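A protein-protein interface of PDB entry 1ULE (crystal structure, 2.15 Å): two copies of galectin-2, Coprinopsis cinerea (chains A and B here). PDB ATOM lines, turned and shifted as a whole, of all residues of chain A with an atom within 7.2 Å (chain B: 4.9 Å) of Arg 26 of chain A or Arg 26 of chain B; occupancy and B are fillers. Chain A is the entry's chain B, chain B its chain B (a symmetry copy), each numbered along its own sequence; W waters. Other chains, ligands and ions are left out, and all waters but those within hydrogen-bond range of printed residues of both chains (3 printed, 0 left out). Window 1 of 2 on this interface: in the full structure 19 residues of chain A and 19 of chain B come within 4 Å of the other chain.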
ATOM      1  N   MET A   1      16.491  36.771  19.533  1.00  0.00           N
ATOM      2  CA  MET A   1      15.910  35.500  20.046  1.00  0.00           C
ATOM      3  C   MET A   1      16.468  34.335  19.246  1.00  0.00           C
ATOM      4  O   MET A   1      16.458  34.355  18.014  1.00  0.00           O
ATOM      5  CB  MET A   1      14.385  35.525  19.925  1.00  0.00           C
ATOM      6  CG  MET A   1      13.687  34.333  20.565  1.00  0.00           C
ATOM      7  SD  MET A   1      13.926  34.214  22.357  1.00  0.00           S
ATOM      8  CE  MET A   1      12.530  35.194  22.935  1.00  0.00           C
ATOM      9  N   LEU A   2      16.958  33.325  19.958  1.00  0.00           N
ATOM     10  CA  LEU A   2      17.538  32.142  19.334  1.00  0.00           C
ATOM     11  C   LEU A   2      16.557  30.981  19.301  1.00  0.00           C
ATOM     12  O   LEU A   2      15.898  30.689  20.297  1.00  0.00           O
ATOM     13  CB  LEU A   2      18.798  31.709  20.096  1.00  0.00           C
ATOM     14  CG  LEU A   2      19.334  30.302  19.795  1.00  0.00           C
ATOM     15  CD1 LEU A   2      19.764  30.196  18.333  1.00  0.00           C
ATOM     16  CD2 LEU A   2      20.509  30.006  20.712  1.00  0.00           C
ATOM     17  N   TYR A   3      16.468  30.322  18.153  1.00  0.00           N
ATOM     18  CA  TYR A   3      15.590  29.165  17.995  1.00  0.00           C
ATOM     19  C   TYR A   3      16.364  28.049  17.324  1.00  0.00           C
ATOM     20  O   TYR A   3      17.280  28.302  16.540  1.00  0.00           O
ATOM     21  CB  TYR A   3      14.382  29.468  17.092  1.00  0.00           C
ATOM     22  CG  TYR A   3      13.486  30.587  17.555  1.00  0.00           C
ATOM     23  CD1 TYR A   3      13.745  31.907  17.188  1.00  0.00           C
ATOM     24  CD2 TYR A   3      12.382  30.328  18.362  1.00  0.00           C
ATOM     25  CE1 TYR A   3      12.920  32.947  17.612  1.00  0.00           C
ATOM     26  CE2 TYR A   3      11.549  31.360  18.798  1.00  0.00           C
ATOM     27  CZ  TYR A   3      11.825  32.669  18.417  1.00  0.00           C
ATOM     28  OH  TYR A   3      11.016  33.698  18.844  1.00  0.00           O
ATOM     29  N   HIS A   4      15.987  26.816  17.638  1.00  0.00           N
ATOM     30  CA  HIS A   4      16.585  25.649  17.011  1.00  0.00           C
ATOM     31  C   HIS A   4      15.450  25.020  16.215  1.00  0.00           C
ATOM     32  O   HIS A   4      14.550  24.397  16.770  1.00  0.00           O
ATOM     33  CB  HIS A   4      17.120  24.687  18.065  1.00  0.00           C
ATOM     34  CG  HIS A   4      18.394  25.150  18.691  1.00  0.00           C
ATOM     35  ND1 HIS A   4      18.593  25.166  20.053  1.00  0.00           N
ATOM     36  CD2 HIS A   4      19.525  25.647  18.137  1.00  0.00           C
ATOM     37  CE1 HIS A   4      19.791  25.658  20.313  1.00  0.00           C
ATOM     38  NE2 HIS A   4      20.378  25.958  19.168  1.00  0.00           N
ATOM     39  N   ALA A  24      18.189  35.218  10.790  1.00  0.00           N
ATOM     40  CA  ALA A  24      19.466  34.698  10.310  1.00  0.00           C
ATOM     41  C   ALA A  24      19.510  33.191  10.557  1.00  0.00           C
ATOM     42  O   ALA A  24      19.656  32.740  11.694  1.00  0.00           O
ATOM     43  CB  ALA A  24      20.628  35.399  11.038  1.00  0.00           C
ATOM     44  N   ILE A  25      19.378  32.428   9.480  1.00  0.00           N
ATOM     45  CA  ILE A  25      19.387  30.972   9.540  1.00  0.00           C
ATOM     46  C   ILE A  25      20.776  30.438   9.214  1.00  0.00           C
ATOM     47  O   ILE A  25      21.337  30.768   8.173  1.00  0.00           O
ATOM     48  CB  ILE A  25      18.399  30.379   8.516  1.00  0.00           C
ATOM     49  CG1 ILE A  25      16.987  30.909   8.780  1.00  0.00           C
ATOM     50  CG2 ILE A  25      18.426  28.860   8.596  1.00  0.00           C
ATOM     51  CD1 ILE A  25      15.974  30.514   7.709  1.00  0.00           C
ATOM     52  N   ARG A  26      21.327  29.611  10.094  1.00  0.00           N
ATOM     53  CA  ARG A  26      22.657  29.051   9.861  1.00  0.00           C
ATOM     54  C   ARG A  26      22.694  27.546  10.110  1.00  0.00           C
ATOM     55  O   ARG A  26      22.147  27.056  11.101  1.00  0.00           O
ATOM     56  CB  ARG A  26      23.681  29.746  10.762  1.00  0.00           C
ATOM     57  CG  ARG A  26      23.749  31.256  10.568  1.00  0.00           C
ATOM     58  CD  ARG A  26      24.896  31.855  11.375  1.00  0.00           C
ATOM     59  NE  ARG A  26      24.656  31.806  12.816  1.00  0.00           N
ATOM     60  CZ  ARG A  26      25.539  31.360  13.706  1.00  0.00           C
ATOM     61  NH1 ARG A  26      26.726  30.909  13.309  1.00  0.00           N
ATOM     62  NH2 ARG A  26      25.243  31.385  14.999  1.00  0.00           N
ATOM     63  N   SER A  27      23.332  26.819   9.200  1.00  0.00           N
ATOM     64  CA  SER A  27      23.452  25.370   9.317  1.00  0.00           C
ATOM     65  C   SER A  27      24.857  24.970   9.755  1.00  0.00           C
ATOM     66  O   SER A  27      25.841  25.566   9.319  1.00  0.00           O
ATOM     67  CB  SER A  27      23.148  24.706   7.976  1.00  0.00           C
ATOM     68  OG  SER A  27      23.475  23.329   8.022  1.00  0.00           O
ATOM     69  N   SER A  28      24.956  23.959  10.611  1.00  0.00           N
ATOM     70  CA  SER A  28      26.264  23.500  11.070  1.00  0.00           C
ATOM     71  C   SER A  28      26.922  22.586  10.038  1.00  0.00           C
ATOM     72  O   SER A  28      28.047  22.134  10.229  1.00  0.00           O
ATOM     73  CB  SER A  28      26.137  22.758  12.405  1.00  0.00           C
ATOM     74  OG  SER A  28      25.157  21.739  12.328  1.00  0.00           O
ATOM     75  N   ALA A  29      26.223  22.326   8.937  1.00  0.00           N
ATOM     76  CA  ALA A  29      26.763  21.450   7.904  1.00  0.00           C
ATOM     77  C   ALA A  29      26.151  21.663   6.527  1.00  0.00           C
ATOM     78  O   ALA A  29      25.147  22.362   6.365  1.00  0.00           O
ATOM     79  CB  ALA A  29      26.577  19.995   8.323  1.00  0.00           C
ATOM     80  N   ASN A  88      29.268  25.780   6.725  1.00  0.00           N
ATOM     81  CA  ASN A  88      28.221  26.459   7.499  1.00  0.00           C
ATOM     82  C   ASN A  88      27.401  27.389   6.600  1.00  0.00           C
ATOM     83  O   ASN A  88      27.489  28.610   6.723  1.00  0.00           O
ATOM     84  CB  ASN A  88      28.840  27.299   8.631  1.00  0.00           C
ATOM     85  CG  ASN A  88      29.524  26.455   9.702  1.00  0.00           C
ATOM     86  OD1 ASN A  88      30.283  26.980  10.516  1.00  0.00           O
ATOM     87  ND2 ASN A  88      29.250  25.154   9.713  1.00  0.00           N
ATOM     88  N   PRO A  89      26.602  26.831   5.677  1.00  0.00           N
ATOM     89  CA  PRO A  89      25.803  27.689   4.796  1.00  0.00           C
ATOM     90  C   PRO A  89      24.732  28.449   5.582  1.00  0.00           C
ATOM     91  O   PRO A  89      24.320  28.011   6.658  1.00  0.00           O
ATOM     92  CB  PRO A  89      25.219  26.698   3.792  1.00  0.00           C
ATOM     93  CG  PRO A  89      25.061  25.462   4.613  1.00  0.00           C
ATOM     94  CD  PRO A  89      26.356  25.408   5.391  1.00  0.00           C
ATOM     95  N   SER A  90      24.288  29.586   5.052  1.00  0.00           N
ATOM     96  CA  SER A  90      23.286  30.392   5.744  1.00  0.00           C
ATOM     97  C   SER A  90      22.250  31.014   4.824  1.00  0.00           C
ATOM     98  O   SER A  90      22.417  31.053   3.602  1.00  0.00           O
ATOM     99  CB  SER A  90      23.963  31.524   6.520  1.00  0.00           C
ATOM    100  OG  SER A  90      24.375  32.557   5.633  1.00  0.00           O
ATOM    101  N   ILE A  91      21.181  31.512   5.440  1.00  0.00           N
ATOM    102  CA  ILE A  91      20.090  32.176   4.735  1.00  0.00           C
ATOM    103  C   ILE A  91      19.612  33.314   5.630  1.00  0.00           C
ATOM    104  O   ILE A  91      19.275  33.098   6.798  1.00  0.00           O
ATOM    105  CB  ILE A  91      18.893  31.223   4.482  1.00  0.00           C
ATOM    106  CG1 ILE A  91      19.323  30.051   3.600  1.00  0.00           C
ATOM    107  CG2 ILE A  91      17.757  31.983   3.794  1.00  0.00           C
ATOM    108  CD1 ILE A  91      18.257  28.992   3.437  1.00  0.00           C
ATOM    109  N   THR A  92      19.602  34.531   5.103  1.00  0.00           N
ATOM    110  CA  THR A  92      19.142  35.661   5.890  1.00  0.00           C
ATOM    111  C   THR A  92      17.899  36.255   5.242  1.00  0.00           C
ATOM    112  O   THR A  92      17.887  36.524   4.044  1.00  0.00           O
ATOM    113  CB  THR A  92      20.229  36.743   6.007  1.00  0.00           C
ATOM    114  OG1 THR A  92      21.399  36.176   6.608  1.00  0.00           O
ATOM    115  CG2 THR A  92      19.737  37.891   6.881  1.00  0.00           C
ATOM    116  N   PHE A 132      20.923  20.753   4.645  1.00  0.00           N
ATOM    117  CA  PHE A 132      21.476  21.353   5.848  1.00  0.00           C
ATOM    118  C   PHE A 132      21.302  20.471   7.074  1.00  0.00           C
ATOM    119  O   PHE A 132      20.736  19.386   6.998  1.00  0.00           O
ATOM    120  CB  PHE A 132      20.804  22.707   6.087  1.00  0.00           C
ATOM    121  CG  PHE A 132      20.773  23.580   4.867  1.00  0.00           C
ATOM    122  CD1 PHE A 132      19.578  24.133   4.423  1.00  0.00           C
ATOM    123  CD2 PHE A 132      21.936  23.825   4.146  1.00  0.00           C
ATOM    124  CE1 PHE A 132      19.541  24.916   3.275  1.00  0.00           C
ATOM    125  CE2 PHE A 132      21.910  24.607   2.996  1.00  0.00           C
ATOM    126  CZ  PHE A 132      20.708  25.154   2.560  1.00  0.00           C
ATOM    127  N   SER A 133      21.784  20.959   8.208  1.00  0.00           N
ATOM    128  CA  SER A 133      21.702  20.219   9.455  1.00  0.00           C
ATOM    129  C   SER A 133      20.326  20.292  10.090  1.00  0.00           C
ATOM    130  O   SER A 133      19.463  21.062   9.672  1.00  0.00           O
ATOM    131  CB  SER A 133      22.729  20.759  10.453  1.00  0.00           C
ATOM    132  OG  SER A 133      22.459  22.119  10.774  1.00  0.00           O
ATOM    133  N   PRO A 135      19.042  20.436  14.088  1.00  0.00           N
ATOM    134  CA  PRO A 135      18.339  21.630  13.609  1.00  0.00           C
ATOM    135  C   PRO A 135      19.277  22.621  12.934  1.00  0.00           C
ATOM    136  O   PRO A 135      20.464  22.347  12.745  1.00  0.00           O
ATOM    137  CB  PRO A 135      17.769  22.209  14.891  1.00  0.00           C
ATOM    138  CG  PRO A 135      18.920  21.971  15.853  1.00  0.00           C
ATOM    139  CD  PRO A 135      19.320  20.536  15.533  1.00  0.00           C
ATOM    140  N   VAL A 136      18.717  23.760  12.544  1.00  0.00           N
ATOM    141  CA  VAL A 136      19.495  24.849  11.976  1.00  0.00           C
ATOM    142  C   VAL A 136      19.353  25.929  13.045  1.00  0.00           C
ATOM    143  O   VAL A 136      18.328  25.997  13.733  1.00  0.00           O
ATOM    144  CB  VAL A 136      18.920  25.375  10.636  1.00  0.00           C
ATOM    145  CG1 VAL A 136      19.045  24.303   9.567  1.00  0.00           C
ATOM    146  CG2 VAL A 136      17.467  25.814  10.808  1.00  0.00           C
ATOM    147  N   THR A 137      20.380  26.748  13.220  1.00  0.00           N
ATOM    148  CA  THR A 137      20.315  27.807  14.213  1.00  0.00           C
ATOM    149  C   THR A 137      19.558  28.989  13.602  1.00  0.00           C
ATOM    150  O   THR A 137      19.804  29.356  12.457  1.00  0.00           O
ATOM    151  CB  THR A 137      21.740  28.246  14.638  1.00  0.00           C
ATOM    152  OG1 THR A 137      22.311  27.244  15.490  1.00  0.00           O
ATOM    153  CG2 THR A 137      21.709  29.571  15.381  1.00  0.00           C
ATOM    154  N   VAL A 138      18.616  29.565  14.345  1.00  0.00           N
ATOM    155  CA  VAL A 138      17.875  30.712  13.835  1.00  0.00           C
ATOM    156  C   VAL A 138      17.854  31.846  14.850  1.00  0.00           C
ATOM    157  O   VAL A 138      17.292  31.709  15.940  1.00  0.00           O
ATOM    158  CB  VAL A 138      16.407  30.354  13.486  1.00  0.00           C
ATOM    159  CG1 VAL A 138      15.741  31.540  12.795  1.00  0.00           C
ATOM    160  CG2 VAL A 138      16.355  29.116  12.589  1.00  0.00           C
ATOM    161  N   ASP A 139      18.494  32.958  14.505  1.00  0.00           N
ATOM    162  CA  ASP A 139      18.502  34.132  15.373  1.00  0.00           C
ATOM    163  C   ASP A 139      17.534  35.137  14.738  1.00  0.00           C
ATOM    164  O   ASP A 139      17.730  35.555  13.600  1.00  0.00           O
ATOM    165  CB  ASP A 139      19.912  34.728  15.464  1.00  0.00           C
ATOM    166  CG  ASP A 139      20.838  33.916  16.371  1.00  0.00           C
ATOM    167  OD1 ASP A 139      20.673  33.981  17.611  1.00  0.00           O
ATOM    168  OD2 ASP A 139      21.725  33.209  15.840  1.00  0.00           O
ATOM    169  N   LEU B   2      30.476  26.951  13.281  1.00  0.00           N
ATOM    170  CA  LEU B   2      29.258  26.655  14.025  1.00  0.00           C
ATOM    171  C   LEU B   2      29.095  25.164  14.275  1.00  0.00           C
ATOM    172  O   LEU B   2      29.280  24.353  13.371  1.00  0.00           O
ATOM    173  CB  LEU B   2      28.032  27.169  13.257  1.00  0.00           C
ATOM    174  CG  LEU B   2      26.665  26.644  13.717  1.00  0.00           C
ATOM    175  CD1 LEU B   2      26.378  27.084  15.151  1.00  0.00           C
ATOM    176  CD2 LEU B   2      25.587  27.168  12.780  1.00  0.00           C
ATOM    177  N   HIS B   4      26.575  22.160  16.525  1.00  0.00           N
ATOM    178  CA  HIS B   4      25.356  21.888  17.269  1.00  0.00           C
ATOM    179  C   HIS B   4      25.731  20.751  18.210  1.00  0.00           C
ATOM    180  O   HIS B   4      25.866  19.602  17.800  1.00  0.00           O
ATOM    181  CB  HIS B   4      24.231  21.480  16.329  1.00  0.00           C
ATOM    182  CG  HIS B   4      23.651  22.629  15.569  1.00  0.00           C
ATOM    183  ND1 HIS B   4      23.446  22.596  14.208  1.00  0.00           N
ATOM    184  CD2 HIS B   4      23.264  23.858  15.982  1.00  0.00           C
ATOM    185  CE1 HIS B   4      22.962  23.760  13.814  1.00  0.00           C
ATOM    186  NE2 HIS B   4      22.843  24.544  14.871  1.00  0.00           N
ATOM    187  N   ALA B  24      31.539  30.380  22.013  1.00  0.00           N
ATOM    188  CA  ALA B  24      30.312  31.017  22.484  1.00  0.00           C
ATOM    189  C   ALA B  24      29.178  29.996  22.444  1.00  0.00           C
ATOM    190  O   ALA B  24      28.684  29.640  21.373  1.00  0.00           O
ATOM    191  CB  ALA B  24      29.976  32.233  21.599  1.00  0.00           C
ATOM    192  N   ILE B  25      28.780  29.531  23.621  1.00  0.00           N
ATOM    193  CA  ILE B  25      27.719  28.543  23.762  1.00  0.00           C
ATOM    194  C   ILE B  25      26.396  29.230  24.075  1.00  0.00           C
ATOM    195  O   ILE B  25      26.310  30.002  25.026  1.00  0.00           O
ATOM    196  CB  ILE B  25      28.031  27.568  24.913  1.00  0.00           C
ATOM    197  CG1 ILE B  25      29.370  26.869  24.663  1.00  0.00           C
ATOM    198  CG2 ILE B  25      26.909  26.548  25.040  1.00  0.00           C
ATOM    199  CD1 ILE B  25      29.845  26.016  25.835  1.00  0.00           C
ATOM    200  N   ARG B  26      25.366  28.949  23.285  1.00  0.00           N
ATOM    201  CA  ARG B  26      24.060  29.563  23.514  1.00  0.00           C
ATOM    202  C   ARG B  26      22.932  28.536  23.472  1.00  0.00           C
ATOM    203  O   ARG B  26      22.895  27.672  22.591  1.00  0.00           O
ATOM    204  CB  ARG B  26      23.804  30.649  22.466  1.00  0.00           C
ATOM    205  CG  ARG B  26      24.861  31.748  22.448  1.00  0.00           C
ATOM    206  CD  ARG B  26      24.456  32.872  21.500  1.00  0.00           C
ATOM    207  NE  ARG B  26      24.501  32.468  20.097  1.00  0.00           N
ATOM    208  CZ  ARG B  26      23.519  32.682  19.225  1.00  0.00           C
ATOM    209  NH1 ARG B  26      22.399  33.290  19.609  1.00  0.00           N
ATOM    210  NH2 ARG B  26      23.664  32.308  17.960  1.00  0.00           N
ATOM    211  N   SER B  27      22.020  28.630  24.433  1.00  0.00           N
ATOM    212  CA  SER B  27      20.883  27.720  24.509  1.00  0.00           C
ATOM    213  C   SER B  27      19.602  28.405  24.049  1.00  0.00           C
ATOM    214  O   SER B  27      19.381  29.579  24.340  1.00  0.00           O
ATOM    215  CB  SER B  27      20.691  27.234  25.944  1.00  0.00           C
ATOM    216  OG  SER B  27      19.468  26.532  26.068  1.00  0.00           O
ATOM    217  N   SER B  28      18.751  27.674  23.335  1.00  0.00           N
ATOM    218  CA  SER B  28      17.492  28.247  22.866  1.00  0.00           C
ATOM    219  C   SER B  28      16.441  28.245  23.974  1.00  0.00           C
ATOM    220  O   SER B  28      15.327  28.727  23.780  1.00  0.00           O
ATOM    221  CB  SER B  28      16.964  27.469  21.655  1.00  0.00           C
ATOM    222  OG  SER B  28      16.907  26.081  21.930  1.00  0.00           O
ATOM    223  N   PRO B  89      19.986  31.486  27.721  1.00  0.00           N
ATOM    224  CA  PRO B  89      21.210  31.610  28.523  1.00  0.00           C
ATOM    225  C   PRO B  89      22.449  31.243  27.705  1.00  0.00           C
ATOM    226  O   PRO B  89      22.352  30.500  26.725  1.00  0.00           O
ATOM    227  CB  PRO B  89      20.955  30.654  29.686  1.00  0.00           C
ATOM    228  CG  PRO B  89      20.120  29.590  29.052  1.00  0.00           C
ATOM    229  CD  PRO B  89      19.144  30.384  28.214  1.00  0.00           C
ATOM    230  N   SER B  90      23.608  31.764  28.098  1.00  0.00           N
ATOM    231  CA  SER B  90      24.840  31.490  27.363  1.00  0.00           C
ATOM    232  C   SER B  90      26.057  31.288  28.249  1.00  0.00           C
ATOM    233  O   SER B  90      26.043  31.603  29.442  1.00  0.00           O
ATOM    234  CB  SER B  90      25.147  32.639  26.401  1.00  0.00           C
ATOM    235  OG  SER B  90      25.662  33.758  27.112  1.00  0.00           O
ATOM    236  N   VAL B 136      22.788  22.764  21.820  1.00  0.00           N
ATOM    237  CA  VAL B 136      23.073  24.141  22.186  1.00  0.00           C
ATOM    238  C   VAL B 136      23.888  24.623  20.988  1.00  0.00           C
ATOM    239  O   VAL B 136      24.603  23.833  20.361  1.00  0.00           O
ATOM    240  CB  VAL B 136      23.928  24.265  23.472  1.00  0.00           C
ATOM    241  CG1 VAL B 136      23.131  23.776  24.670  1.00  0.00           C
ATOM    242  CG2 VAL B 136      25.235  23.488  23.328  1.00  0.00           C
ATOM    243  N   THR B 137      23.763  25.896  20.642  1.00  0.00           N
ATOM    244  CA  THR B 137      24.516  26.430  19.520  1.00  0.00           C
ATOM    245  C   THR B 137      25.926  26.767  20.006  1.00  0.00           C
ATOM    246  O   THR B 137      26.090  27.351  21.073  1.00  0.00           O
ATOM    247  CB  THR B 137      23.826  27.700  18.955  1.00  0.00           C
ATOM    248  OG1 THR B 137      22.658  27.317  18.216  1.00  0.00           O
ATOM    249  CG2 THR B 137      24.763  28.472  18.041  1.00  0.00           C
ATOM    250  N   ASP B 139      29.475  28.561  18.632  1.00  0.00           N
ATOM    251  CA  ASP B 139      30.268  29.243  17.612  1.00  0.00           C
ATOM    252  C   ASP B 139      31.698  29.311  18.159  1.00  0.00           C
ATOM    253  O   ASP B 139      31.932  29.891  19.217  1.00  0.00           O
ATOM    254  CB  ASP B 139      29.722  30.653  17.357  1.00  0.00           C
ATOM    255  CG  ASP B 139      28.445  30.649  16.516  1.00  0.00           C
ATOM    256  OD1 ASP B 139      28.532  30.404  15.291  1.00  0.00           O
ATOM    257  OD2 ASP B 139      27.354  30.884  17.086  1.00  0.00           O
HETATM  258  O   HOH W   1      29.621  21.881  12.425  1.00  0.00           O
HETATM  259  O   HOH W   2      13.931  29.391  21.549  1.00  0.00           O
HETATM  260  O   HOH W   3      22.288  19.719  13.947  1.00  0.00           O
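Among the printed residues, pairs that only touch across the chains: Ser 133 of chain A with His 4 of chain B (3.5 Å), Leu 2 of chain A with Ser 28 of chain B (3.7 Å), Ser 28 of chain A with Leu 2 of chain B (3.7 Å), Leu 2 of chain A with Arg 26 of chain B (3.8 Å), Arg 26 of chain A with Leu 2 of chain B (3.8 Å), Ser 27 of chain A with Leu 2 of chain B (3.8 Å) and Leu 2 of chain A with Ser 27 of chain B (3.8 Å).
NH2 of Arg 26 of chain A lies close to NH2 of Arg 26 of chain B, 3.5 Å away.
The side-chain carboxylate (OD1) of Asp 139 of chain B lies within salt-bridge range of the guanidinium group (NH1) of Arg 26 of chain A, 2.7 Å away.
ND1 of His 4 of chain B sits close to O of Pro 135 of chain A.
NE2 of His 4 of chain B is in hydrogen-bond range of OG1 of Thr 137 of chain A (2.8 Å).
A ring nitrogen (ND1) of His 4 of chain A lies within hydrogen-bond range of the side-chain hydroxyl (OG) of Ser 28 of chain B, 2.7 Å away.
The side-chain hydroxyl of Ser 28 of chain A lies within hydrogen-bond range of a ring nitrogen (ND1) of His 4 of chain B, at 2.7 Å.
A ring nitrogen (NE2) of His 4 of chain A is in hydrogen-bond range of the side-chain hydroxyl of Thr 137 of chain B, 2.8 Å away.
The side-chain hydroxyl (OG1) of Thr 137 of chain B lies within hydrogen-bond range of the side-chain hydroxyl (OG1) of Thr 137 of chain A, at 2.7 Å.
The guanidinium group (NH1) of Arg 26 of chain B lies within salt-bridge range of the side-chain carboxylate (OD1) of Asp 139 of chain A, 2.7 Å away.
The backbone NH (N) of Leu 2 of chain B lies within hydrogen-bond range of the side-chain amide oxygen (OD1) of Asn 88 of chain A (2.8 Å).
Of the 12 printed residues of chain B, 7 touch a printed residue of chain A.
Hydrophobic or aromatic side chains of chain B that line the printed part of chain A: Leu 2 and His 4.
Printed residues of chain A that touch a printed residue of chain B: Leu 2, His 4, Arg 26, Ser 27, Ser 28, Asn 88, Ser 133, Pro 135, Thr 137 and Asp 139.
Among the printed residues, 17 pairs touch across the chains.
Leu 2 of chain A touches Arg 26 of chain B, and with the chains exchanged Arg 26 of chain A touches Leu 2 of chain B.
Leu 2 of chain A touches Ser 27 of chain B, and with the chains exchanged Ser 27 of chain A touches Leu 2 of chain B.
His 4 of chain A touches Ser 28 of chain B, and with the chains exchanged Ser 28 of chain A touches His 4 of chain B.
Arg 26 of chain B touches its own counterpart, Arg 26 of chain A.
Positions printed for both chains: 2, 4, 24, 25, 26, 27, 28, 89, 90, 136, 137 and 139.
Of the 17 pairs that touch across the chains among the printed residues, 14 have their exchanged pair printed and touching as well.
Water W2 lies within hydrogen-bond range of the backbone carbonyl oxygen of Leu 2 of chain A (2.7 Å) and the backbone carbonyl oxygen of Ser 28 of chain B (2.7 Å).
Water W1 bridges the backbone carbonyl oxygen of Leu 2 of chain B (2.7 Å) and the backbone carbonyl oxygen of Ser 28 of chain A (2.7 Å).
Water W3 lies within hydrogen-bond range of a ring nitrogen (ND1) of His 4 of chain B (3.1 Å) and the backbone carbonyl oxygen (O) of Pro 135 of chain A (3.4 Å).
The side-chain hydroxyl (OG) of Ser 27 of chain A is in hydrogen-bond range of the backbone carbonyl oxygen (O) of Ala 29 of chain A, 2.5 Å away.
The backbone carbonyl oxygen of Pro 89 of chain B sits at hydrogen-bond distance from the backbone NH of Ser 27 of chain B, at 3.0 Å.
The backbone carbonyl oxygen of Ser 27 of chain A sits close to the side-chain amide nitrogen of Asn 88 of chain A (3.5 Å).
The side-chain amide nitrogen (ND2) of Asn 88 of chain A is in hydrogen-bond range of the backbone carbonyl oxygen (O) of Ser 28 of chain A (3.3 Å).
The backbone NH of Ser 27 of chain A sits at hydrogen-bond distance from the backbone carbonyl oxygen of Pro 89 of chain A (3.0 Å).
N of Ser 28 of chain A lies within hydrogen-bond range of OG of Ser 133 of chain A.
Of chain B, only Leu 2 (3.8 Å), Arg 26 (3.5 Å) and Asp 139 (2.7 Å) come within 4 Å of Arg 26 of chain A.
Of the printed residues of chain B, Asn 88 of chain A touches Leu 2 (2.8 Å).
Thr 92 of chain A touches none of the printed residues of chain B.
Printed residues of chain B within 4 Å of Ser 133 of chain A: His 4 (3.5 Å).
Of the printed residues of chain B, Thr 137 of chain A touches His 4 (2.8 Å) and Thr 137 (2.7 Å).
Of the printed residues of chain A, Leu 2 of chain B touches Arg 26, Ser 27, Ser 28 and Asn 88.
Of chain A, only Leu 2, Arg 26 and Asp 139 come within 4 Å of Arg 26 of chain B.
Of the printed residues of chain A, Ser 27 of chain B touches Leu 2.
The nearest residue of chain B that does not touch Arg 26 of chain A is Thr 137 of chain B (4.2 Å).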
